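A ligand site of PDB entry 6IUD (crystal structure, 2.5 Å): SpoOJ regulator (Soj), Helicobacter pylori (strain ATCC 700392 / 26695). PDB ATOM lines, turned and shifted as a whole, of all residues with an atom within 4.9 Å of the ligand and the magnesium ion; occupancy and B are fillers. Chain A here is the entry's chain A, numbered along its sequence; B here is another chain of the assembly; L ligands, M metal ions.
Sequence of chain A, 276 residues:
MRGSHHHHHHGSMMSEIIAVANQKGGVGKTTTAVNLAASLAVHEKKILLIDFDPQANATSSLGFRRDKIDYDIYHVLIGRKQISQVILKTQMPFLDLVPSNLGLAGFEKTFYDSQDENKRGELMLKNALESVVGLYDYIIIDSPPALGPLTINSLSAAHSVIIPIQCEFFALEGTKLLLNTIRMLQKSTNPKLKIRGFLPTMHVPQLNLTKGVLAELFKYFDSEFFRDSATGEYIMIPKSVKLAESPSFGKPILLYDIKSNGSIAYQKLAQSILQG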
ATOM      1  N   LYS A  24      10.505  -9.873   9.573  1.00  0.00           N
ATOM      2  CA  LYS A  24      11.821  -9.258   9.665  1.00  0.00           C
ATOM      3  C   LYS A  24      12.243  -8.716   8.295  1.00  0.00           C
ATOM      4  O   LYS A  24      12.028  -9.344   7.255  1.00  0.00           O
ATOM      5  CB  LYS A  24      12.844 -10.284  10.199  1.00  0.00           C
ATOM      6  CG  LYS A  24      14.188  -9.717  10.565  1.00  0.00           C
ATOM      7  CD  LYS A  24      14.608  -9.789  12.057  1.00  0.00           C
ATOM      8  CE  LYS A  24      15.810  -8.824  12.324  1.00  0.00           C
ATOM      9  NZ  LYS A  24      15.439  -7.440  11.875  1.00  0.00           N
ATOM     10  N   GLY A  25      12.863  -7.544   8.294  1.00  0.00           N
ATOM     11  CA  GLY A  25      13.361  -6.977   7.071  1.00  0.00           C
ATOM     12  C   GLY A  25      14.807  -7.313   6.839  1.00  0.00           C
ATOM     13  O   GLY A  25      15.517  -7.680   7.802  1.00  0.00           O
ATOM     14  N   GLY A  26      15.212  -7.189   5.576  1.00  0.00           N
ATOM     15  CA  GLY A  26      16.551  -7.495   5.111  1.00  0.00           C
ATOM     16  C   GLY A  26      16.919  -8.966   5.055  1.00  0.00           C
ATOM     17  O   GLY A  26      18.101  -9.289   5.150  1.00  0.00           O
ATOM     18  N   VAL A  27      15.942  -9.876   4.975  1.00  0.00           N
ATOM     19  CA  VAL A  27      16.238 -11.307   5.080  1.00  0.00           C
ATOM     20  C   VAL A  27      16.168 -12.024   3.738  1.00  0.00           C
ATOM     21  O   VAL A  27      16.280 -13.257   3.717  1.00  0.00           O
ATOM     22  CB  VAL A  27      15.314 -12.035   6.096  1.00  0.00           C
ATOM     23  CG1 VAL A  27      15.298 -11.301   7.500  1.00  0.00           C
ATOM     24  CG2 VAL A  27      13.936 -12.207   5.547  1.00  0.00           C
ATOM     25  N   GLY A  28      15.967 -11.295   2.636  1.00  0.00           N
ATOM     26  CA  GLY A  28      15.933 -11.906   1.323  1.00  0.00           C
ATOM     27  C   GLY A  28      14.579 -12.204   0.729  1.00  0.00           C
ATOM     28  O   GLY A  28      14.508 -12.968  -0.254  1.00  0.00           O
ATOM     29  N   LYS A  29      13.486 -11.604   1.219  1.00  0.00           N
ATOM     30  CA  LYS A  29      12.170 -11.909   0.644  1.00  0.00           C
ATOM     31  C   LYS A  29      12.101 -11.448  -0.808  1.00  0.00           C
ATOM     32  O   LYS A  29      11.679 -12.193  -1.694  1.00  0.00           O
ATOM     33  CB  LYS A  29      11.057 -11.226   1.437  1.00  0.00           C
ATOM     34  CG  LYS A  29      10.980 -11.735   2.889  1.00  0.00           C
ATOM     35  CD  LYS A  29       9.878 -10.999   3.637  1.00  0.00           C
ATOM     36  CE  LYS A  29      10.089  -9.467   3.558  1.00  0.00           C
ATOM     37  NZ  LYS A  29      11.084  -8.948   4.503  1.00  0.00           N
ATOM     38  N   THR A  30      12.523 -10.206  -1.062  1.00  0.00           N
ATOM     39  CA  THR A  30      12.357  -9.669  -2.409  1.00  0.00           C
ATOM     40  C   THR A  30      13.301 -10.349  -3.380  1.00  0.00           C
ATOM     41  O   THR A  30      12.907 -10.730  -4.478  1.00  0.00           O
ATOM     42  CB  THR A  30      12.596  -8.139  -2.366  1.00  0.00           C
ATOM     43  OG1 THR A  30      11.685  -7.538  -1.424  1.00  0.00           O
ATOM     44  CG2 THR A  30      12.409  -7.546  -3.745  1.00  0.00           C
ATOM     45  N   THR A  31      14.539 -10.615  -2.945  1.00  0.00           N
ATOM     46  CA  THR A  31      15.494 -11.344  -3.751  1.00  0.00           C
ATOM     47  C   THR A  31      14.966 -12.728  -4.117  1.00  0.00           C
ATOM     48  O   THR A  31      15.066 -13.155  -5.276  1.00  0.00           O
ATOM     49  CB  THR A  31      16.808 -11.448  -2.973  1.00  0.00           C
ATOM     50  OG1 THR A  31      17.261 -10.138  -2.643  1.00  0.00           O
ATOM     51  CG2 THR A  31      17.894 -12.137  -3.752  1.00  0.00           C
ATOM     52  N   ASP A  53       4.698  -4.664  -1.389  1.00  0.00           N
ATOM     53  CA  ASP A  53       5.418  -3.850  -0.450  1.00  0.00           C
ATOM     54  C   ASP A  53       5.488  -2.427  -0.968  1.00  0.00           C
ATOM     55  O   ASP A  53       5.927  -2.212  -2.111  1.00  0.00           O
ATOM     56  CB  ASP A  53       6.813  -4.438  -0.229  1.00  0.00           C
ATOM     57  CG  ASP A  53       7.649  -3.623   0.719  1.00  0.00           C
ATOM     58  OD1 ASP A  53       8.788  -4.042   1.022  1.00  0.00           O
ATOM     59  OD2 ASP A  53       7.143  -2.586   1.211  1.00  0.00           O
ATOM     60  N   GLN A  55       7.481   0.168  -0.610  1.00  0.00           N
ATOM     61  CA  GLN A  55       8.775   0.617  -1.138  1.00  0.00           C
ATOM     62  C   GLN A  55       9.040   0.025  -2.517  1.00  0.00           C
ATOM     63  O   GLN A  55       9.720   0.652  -3.346  1.00  0.00           O
ATOM     64  CB  GLN A  55       9.902   0.281  -0.147  1.00  0.00           C
ATOM     65  CG  GLN A  55       9.833  -1.144   0.454  1.00  0.00           C
ATOM     66  CD  GLN A  55      11.099  -1.514   1.220  1.00  0.00           C
ATOM     67  OE1 GLN A  55      12.054  -0.743   1.221  1.00  0.00           O
ATOM     68  NE2 GLN A  55      11.124  -2.723   1.853  1.00  0.00           N
ATOM     69  N   ASN A  57      10.539  -2.876  -3.931  1.00  0.00           N
ATOM     70  CA  ASN A  57      11.833  -3.323  -4.439  1.00  0.00           C
ATOM     71  C   ASN A  57      11.708  -4.347  -5.551  1.00  0.00           C
ATOM     72  O   ASN A  57      12.521  -4.339  -6.479  1.00  0.00           O
ATOM     73  CB  ASN A  57      12.689  -3.902  -3.321  1.00  0.00           C
ATOM     74  CG  ASN A  57      13.112  -2.861  -2.275  1.00  0.00           C
ATOM     75  OD1 ASN A  57      12.948  -1.638  -2.435  1.00  0.00           O
ATOM     76  ND2 ASN A  57      13.735  -3.359  -1.211  1.00  0.00           N
ATOM     77  N   ASP A 142       5.368 -10.915  -2.961  1.00  0.00           N
ATOM     78  CA  ASP A 142       6.548 -10.470  -2.235  1.00  0.00           C
ATOM     79  C   ASP A 142       6.049  -9.558  -1.128  1.00  0.00           C
ATOM     80  O   ASP A 142       5.512  -8.470  -1.396  1.00  0.00           O
ATOM     81  CB  ASP A 142       7.542  -9.766  -3.162  1.00  0.00           C
ATOM     82  CG  ASP A 142       8.690  -9.113  -2.405  1.00  0.00           C
ATOM     83  OD1 ASP A 142       9.062  -9.624  -1.314  1.00  0.00           O
ATOM     84  OD2 ASP A 142       9.240  -8.124  -2.958  1.00  0.00           O
ATOM     85  N   SER A 143       6.221 -10.020   0.174  1.00  0.00           N
ATOM     86  CA  SER A 143       5.520  -9.355   1.249  1.00  0.00           C
ATOM     87  C   SER A 143       6.404  -8.298   1.897  1.00  0.00           C
ATOM     88  O   SER A 143       7.633  -8.344   1.778  1.00  0.00           O
ATOM     89  CB  SER A 143       5.071 -10.388   2.291  1.00  0.00           C
ATOM     90  OG  SER A 143       4.568 -11.544   1.651  1.00  0.00           O
ATOM     91  N   MET A 202      21.432 -15.654   2.363  1.00  0.00           N
ATOM     92  CA  MET A 202      22.698 -15.008   2.735  1.00  0.00           C
ATOM     93  C   MET A 202      23.531 -15.937   3.611  1.00  0.00           C
ATOM     94  O   MET A 202      24.188 -15.511   4.564  1.00  0.00           O
ATOM     95  CB  MET A 202      22.435 -13.687   3.408  1.00  0.00           C
ATOM     96  CG  MET A 202      21.418 -12.913   2.626  1.00  0.00           C
ATOM     97  SD  MET A 202      21.423 -11.205   3.027  1.00  0.00           S
ATOM     98  CE  MET A 202      19.905 -11.230   3.884  1.00  0.00           C
ATOM     99  N   ILE A 237      20.359 -20.326  -0.238  1.00  0.00           N
ATOM    100  CA  ILE A 237      20.933 -19.246  -1.047  1.00  0.00           C
ATOM    101  C   ILE A 237      22.213 -18.760  -0.405  1.00  0.00           C
ATOM    102  O   ILE A 237      22.189 -18.192   0.703  1.00  0.00           O
ATOM    103  CB  ILE A 237      19.947 -18.096  -1.189  1.00  0.00           C
ATOM    104  CG1 ILE A 237      18.538 -18.664  -1.353  1.00  0.00           C
ATOM    105  CG2 ILE A 237      20.425 -17.151  -2.303  1.00  0.00           C
ATOM    106  CD1 ILE A 237      18.331 -19.536  -2.588  1.00  0.00           C
ATOM    107  N   PRO A 238      23.347 -18.906  -1.086  1.00  0.00           N
ATOM    108  CA  PRO A 238      24.603 -18.432  -0.502  1.00  0.00           C
ATOM    109  C   PRO A 238      24.633 -16.913  -0.484  1.00  0.00           C
ATOM    110  O   PRO A 238      23.999 -16.255  -1.300  1.00  0.00           O
ATOM    111  CB  PRO A 238      25.672 -19.024  -1.423  1.00  0.00           C
ATOM    112  CG  PRO A 238      24.992 -19.236  -2.675  1.00  0.00           C
ATOM    113  CD  PRO A 238      23.520 -19.427  -2.441  1.00  0.00           C
ATOM    114  N   LYS A 239      25.360 -16.359   0.466  1.00  0.00           N
ATOM    115  CA  LYS A 239      25.625 -14.935   0.403  1.00  0.00           C
ATOM    116  C   LYS A 239      26.559 -14.675  -0.784  1.00  0.00           C
ATOM    117  O   LYS A 239      27.639 -15.274  -0.873  1.00  0.00           O
ATOM    118  CB  LYS A 239      26.206 -14.412   1.717  1.00  0.00           C
ATOM    119  CG  LYS A 239      26.448 -12.879   1.657  1.00  0.00           C
ATOM    120  CD  LYS A 239      26.807 -12.169   2.991  1.00  0.00           C
ATOM    121  CE  LYS A 239      25.710 -11.133   3.350  1.00  0.00           C
ATOM    122  NZ  LYS A 239      25.337 -10.959   4.791  1.00  0.00           N
ATOM    123  N   SER A 240      26.153 -13.761  -1.674  1.00  0.00           N
ATOM    124  CA  SER A 240      26.789 -13.579  -2.976  1.00  0.00           C
ATOM    125  C   SER A 240      26.580 -12.116  -3.387  1.00  0.00           C
ATOM    126  O   SER A 240      25.449 -11.676  -3.562  1.00  0.00           O
ATOM    127  CB  SER A 240      26.195 -14.537  -4.028  1.00  0.00           C
ATOM    128  OG  SER A 240      26.551 -14.193  -5.359  1.00  0.00           O
ATOM    129  N   VAL A 241      27.670 -11.356  -3.487  1.00  0.00           N
ATOM    130  CA  VAL A 241      27.512  -9.987  -3.944  1.00  0.00           C
ATOM    131  C   VAL A 241      26.879  -9.916  -5.347  1.00  0.00           C
ATOM    132  O   VAL A 241      26.304  -8.865  -5.690  1.00  0.00           O
ATOM    133  CB  VAL A 241      28.811  -9.191  -3.924  1.00  0.00           C
ATOM    134  CG1 VAL A 241      29.574  -9.449  -5.177  1.00  0.00           C
ATOM    135  CG2 VAL A 241      28.483  -7.661  -3.728  1.00  0.00           C
ATOM    136  N   LEU A 243      24.232 -11.467  -6.235  1.00  0.00           N
ATOM    137  CA  LEU A 243      22.795 -11.329  -6.028  1.00  0.00           C
ATOM    138  C   LEU A 243      22.452  -9.939  -5.526  1.00  0.00           C
ATOM    139  O   LEU A 243      21.326  -9.473  -5.739  1.00  0.00           O
ATOM    140  CB  LEU A 243      22.233 -12.342  -5.055  1.00  0.00           C
ATOM    141  CG  LEU A 243      22.142 -13.773  -5.549  1.00  0.00           C
ATOM    142  CD1 LEU A 243      22.064 -14.678  -4.337  1.00  0.00           C
ATOM    143  CD2 LEU A 243      20.949 -13.900  -6.491  1.00  0.00           C
ATOM    144  N   ALA A 244      23.381  -9.274  -4.857  1.00  0.00           N
ATOM    145  CA  ALA A 244      23.052  -7.920  -4.427  1.00  0.00           C
ATOM    146  C   ALA A 244      23.205  -6.911  -5.558  1.00  0.00           C
ATOM    147  O   ALA A 244      22.428  -5.946  -5.640  1.00  0.00           O
ATOM    148  CB  ALA A 244      23.887  -7.528  -3.203  1.00  0.00           C
ATOM    149  N   PRO A 247      19.772  -6.299  -8.765  1.00  0.00           N
ATOM    150  CA  PRO A 247      18.764  -5.247  -8.961  1.00  0.00           C
ATOM    151  C   PRO A 247      19.326  -4.010  -9.636  1.00  0.00           C
ATOM    152  O   PRO A 247      18.571  -3.272 -10.280  1.00  0.00           O
ATOM    153  CB  PRO A 247      18.329  -4.944  -7.526  1.00  0.00           C
ATOM    154  CG  PRO A 247      19.516  -5.341  -6.690  1.00  0.00           C
ATOM    155  CD  PRO A 247      19.925  -6.622  -7.342  1.00  0.00           C
ATOM    156  N   LYS B  24      14.053   1.022   5.680  1.00  0.00           N
ATOM    157  CA  LYS B  24      14.361  -0.411   5.590  1.00  0.00           C
ATOM    158  C   LYS B  24      14.720  -1.081   6.914  1.00  0.00           C
ATOM    159  O   LYS B  24      15.393  -0.503   7.769  1.00  0.00           O
ATOM    160  CB  LYS B  24      15.531  -0.712   4.657  1.00  0.00           C
ATOM    161  CG  LYS B  24      15.505  -2.157   4.158  1.00  0.00           C
ATOM    162  CD  LYS B  24      16.062  -2.529   2.842  1.00  0.00           C
ATOM    163  CE  LYS B  24      15.994  -4.009   2.765  1.00  0.00           C
ATOM    164  NZ  LYS B  24      14.613  -4.382   2.562  1.00  0.00           N
ATOM    165  N   GLN B 166      23.175   0.512   5.368  1.00  0.00           N
ATOM    166  CA  GLN B 166      23.842  -0.607   4.745  1.00  0.00           C
ATOM    167  C   GLN B 166      24.029  -0.257   3.267  1.00  0.00           C
ATOM    168  O   GLN B 166      23.069   0.091   2.590  1.00  0.00           O
ATOM    169  CB  GLN B 166      22.979  -1.866   4.935  1.00  0.00           C
ATOM    170  CG  GLN B 166      23.235  -2.877   3.923  1.00  0.00           C
ATOM    171  CD  GLN B 166      22.508  -4.147   4.210  1.00  0.00           C
ATOM    172  OE1 GLN B 166      23.149  -5.187   4.323  1.00  0.00           O
ATOM    173  NE2 GLN B 166      21.190  -4.092   4.338  1.00  0.00           N
ATOM    174  N   GLU B 168      23.949  -0.971   0.078  1.00  0.00           N
ATOM    175  CA  GLU B 168      23.556  -1.845  -1.029  1.00  0.00           C
ATOM    176  C   GLU B 168      22.690  -0.968  -1.918  1.00  0.00           C
ATOM    177  O   GLU B 168      22.340   0.147  -1.565  1.00  0.00           O
ATOM    178  CB  GLU B 168      22.588  -2.972  -0.638  1.00  0.00           C
ATOM    179  CG  GLU B 168      21.497  -2.362   0.145  1.00  0.00           C
ATOM    180  CD  GLU B 168      20.244  -2.416  -0.756  1.00  0.00           C
ATOM    181  OE1 GLU B 168      20.363  -2.759  -1.976  1.00  0.00           O
ATOM    182  OE2 GLU B 168      19.295  -1.663  -0.433  1.00  0.00           O
HETATM  183  P1  LIG L   1      13.662  -8.128   2.090  1.00  0.00           P
HETATM  184  O1  LIG L   1      12.775  -8.101   0.887  1.00  0.00           O
HETATM  185  O2  LIG L   1      13.467  -9.326   2.966  1.00  0.00           O
HETATM  186  O3  LIG L   1      13.691  -6.817   2.827  1.00  0.00           O
HETATM  187  P2  LIG L   1      15.848  -8.137   0.242  1.00  0.00           P
HETATM  188  O4  LIG L   1      15.573  -9.265  -0.678  1.00  0.00           O
HETATM  189  O5  LIG L   1      15.552  -6.688  -0.151  1.00  0.00           O
HETATM  190  O6  LIG L   1      15.145  -8.523   1.645  1.00  0.00           O
HETATM  191  O7  LIG L   1      17.409  -8.206   0.664  1.00  0.00           O
HETATM  192  C1  LIG L   1      18.048  -7.317   1.587  1.00  0.00           C
HETATM  193  C2  LIG L   1      19.385  -6.876   1.028  1.00  0.00           C
HETATM  194  O8  LIG L   1      20.213  -8.026   0.921  1.00  0.00           O
HETATM  195  C3  LIG L   1      19.361  -6.367  -0.398  1.00  0.00           C
HETATM  196  O9  LIG L   1      20.535  -5.586  -0.443  1.00  0.00           O
HETATM  197  C4  LIG L   1      19.636  -7.574  -1.265  1.00  0.00           C
HETATM  198  O10 LIG L   1      20.142  -7.327  -2.575  1.00  0.00           O
HETATM  199  C5  LIG L   1      20.672  -8.250  -0.419  1.00  0.00           C
HETATM  200  N1  LIG L   1      20.710  -9.712  -0.623  1.00  0.00           N
HETATM  201  C6  LIG L   1      19.636 -10.523  -0.730  1.00  0.00           C
HETATM  202  N2  LIG L   1      20.028 -11.818  -0.849  1.00  0.00           N
HETATM  203  C7  LIG L   1      21.390 -11.836  -0.838  1.00  0.00           C
HETATM  204  C8  LIG L   1      22.477 -12.872  -0.920  1.00  0.00           C
HETATM  205  N3  LIG L   1      22.175 -14.207  -1.046  1.00  0.00           N
HETATM  206  N4  LIG L   1      23.768 -12.445  -0.860  1.00  0.00           N
HETATM  207  C9  LIG L   1      24.066 -11.148  -0.707  1.00  0.00           C
HETATM  208  N5  LIG L   1      23.140 -10.178  -0.630  1.00  0.00           N
HETATM  209  C10 LIG L   1      21.823 -10.437  -0.703  1.00  0.00           C
HETATM  210 MG    MG M   1      11.432  -6.215   0.391  1.00  0.00          MG
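O4 of the ligand is in hydrogen-bond range of N of Thr 30, at 3.2 Å.
NZ of Lys 24 of chain B is in salt-bridge range of O3 of the ligand (2.6 Å).
The backbone NH (N) of Thr 31 is in hydrogen-bond range of an oxygen (O4) of the ligand.
OG1 of Thr 31 lies within hydrogen-bond range of O4 of the ligand, at 2.7 Å.
A nitrogen (N3) of the ligand is in hydrogen-bond range of the backbone carbonyl oxygen of Pro 238, at 2.8 Å.
The backbone NH (N) of Ser 240 is in hydrogen-bond range of a nitrogen (N4) of the ligand (2.8 Å).
N of Lys 29 lies within hydrogen-bond range of O2 of the ligand (2.9 Å).
The side-chain amino group of Lys 29 lies within salt-bridge range of an oxygen (O2) of the ligand.
The backbone NH (N) of Gly 28 lies within hydrogen-bond range of an oxygen (O6) of the ligand (3.1 Å).
The backbone NH (N) of Gly 26 sits at hydrogen-bond distance from an oxygen (O3) of the ligand, 3.2 Å away.
The side-chain carboxylate (OE1) of Glu 168 of chain B sits close to an oxygen (O9) of the ligand, at 3.2 Å.
The backbone NH of Val 27 is in hydrogen-bond range of an oxygen (O2) of the ligand.
Residues that only touch the ligand: Leu 243, Lys 239, Ala 244, Met 202, Ile 237 and Asn 57.
Hydrophobic or aromatic side chains within 4 Å of the ligand: Val 27, Met 202, Ile 237, Leu 243 and Ala 244.
Of the 25 residues printed, 16 come within 4 Å of the ligand.
The nearest printed residue that does not touch the ligand is Gly 25 (4.2 Å).
The side-chain hydroxyl (OG1) of Thr 30 sits close to the side-chain carboxylate (OD2) of Asp 142, at 2.9 Å.
NZ of Lys 29 sits at hydrogen-bond distance from O of Lys 24 of chain A (2.9 Å).
OD1 of Asp 53 sits at hydrogen-bond distance from NE2 of Gln 55, 2.8 Å away.
N of Met 202 sits at hydrogen-bond distance from O of Ile 237, at 3.1 Å.
The magnesium ion is bound by the side-chain hydroxyl (OG1) of Thr 30, at 2.3 Å.
An oxygen (O1) of the ligand binds the magnesium ion (2.4 Å).
The magnesium ion has two donor atoms within binding distance.
Merely in contact with the magnesium ion: Asp 53 and Gln 55.
Of the 25 residues printed, 3 come within 4 Å of the magnesium ion.
Along chain A the residues within 4 Å of the magnesium ion span positions 30 to 55.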
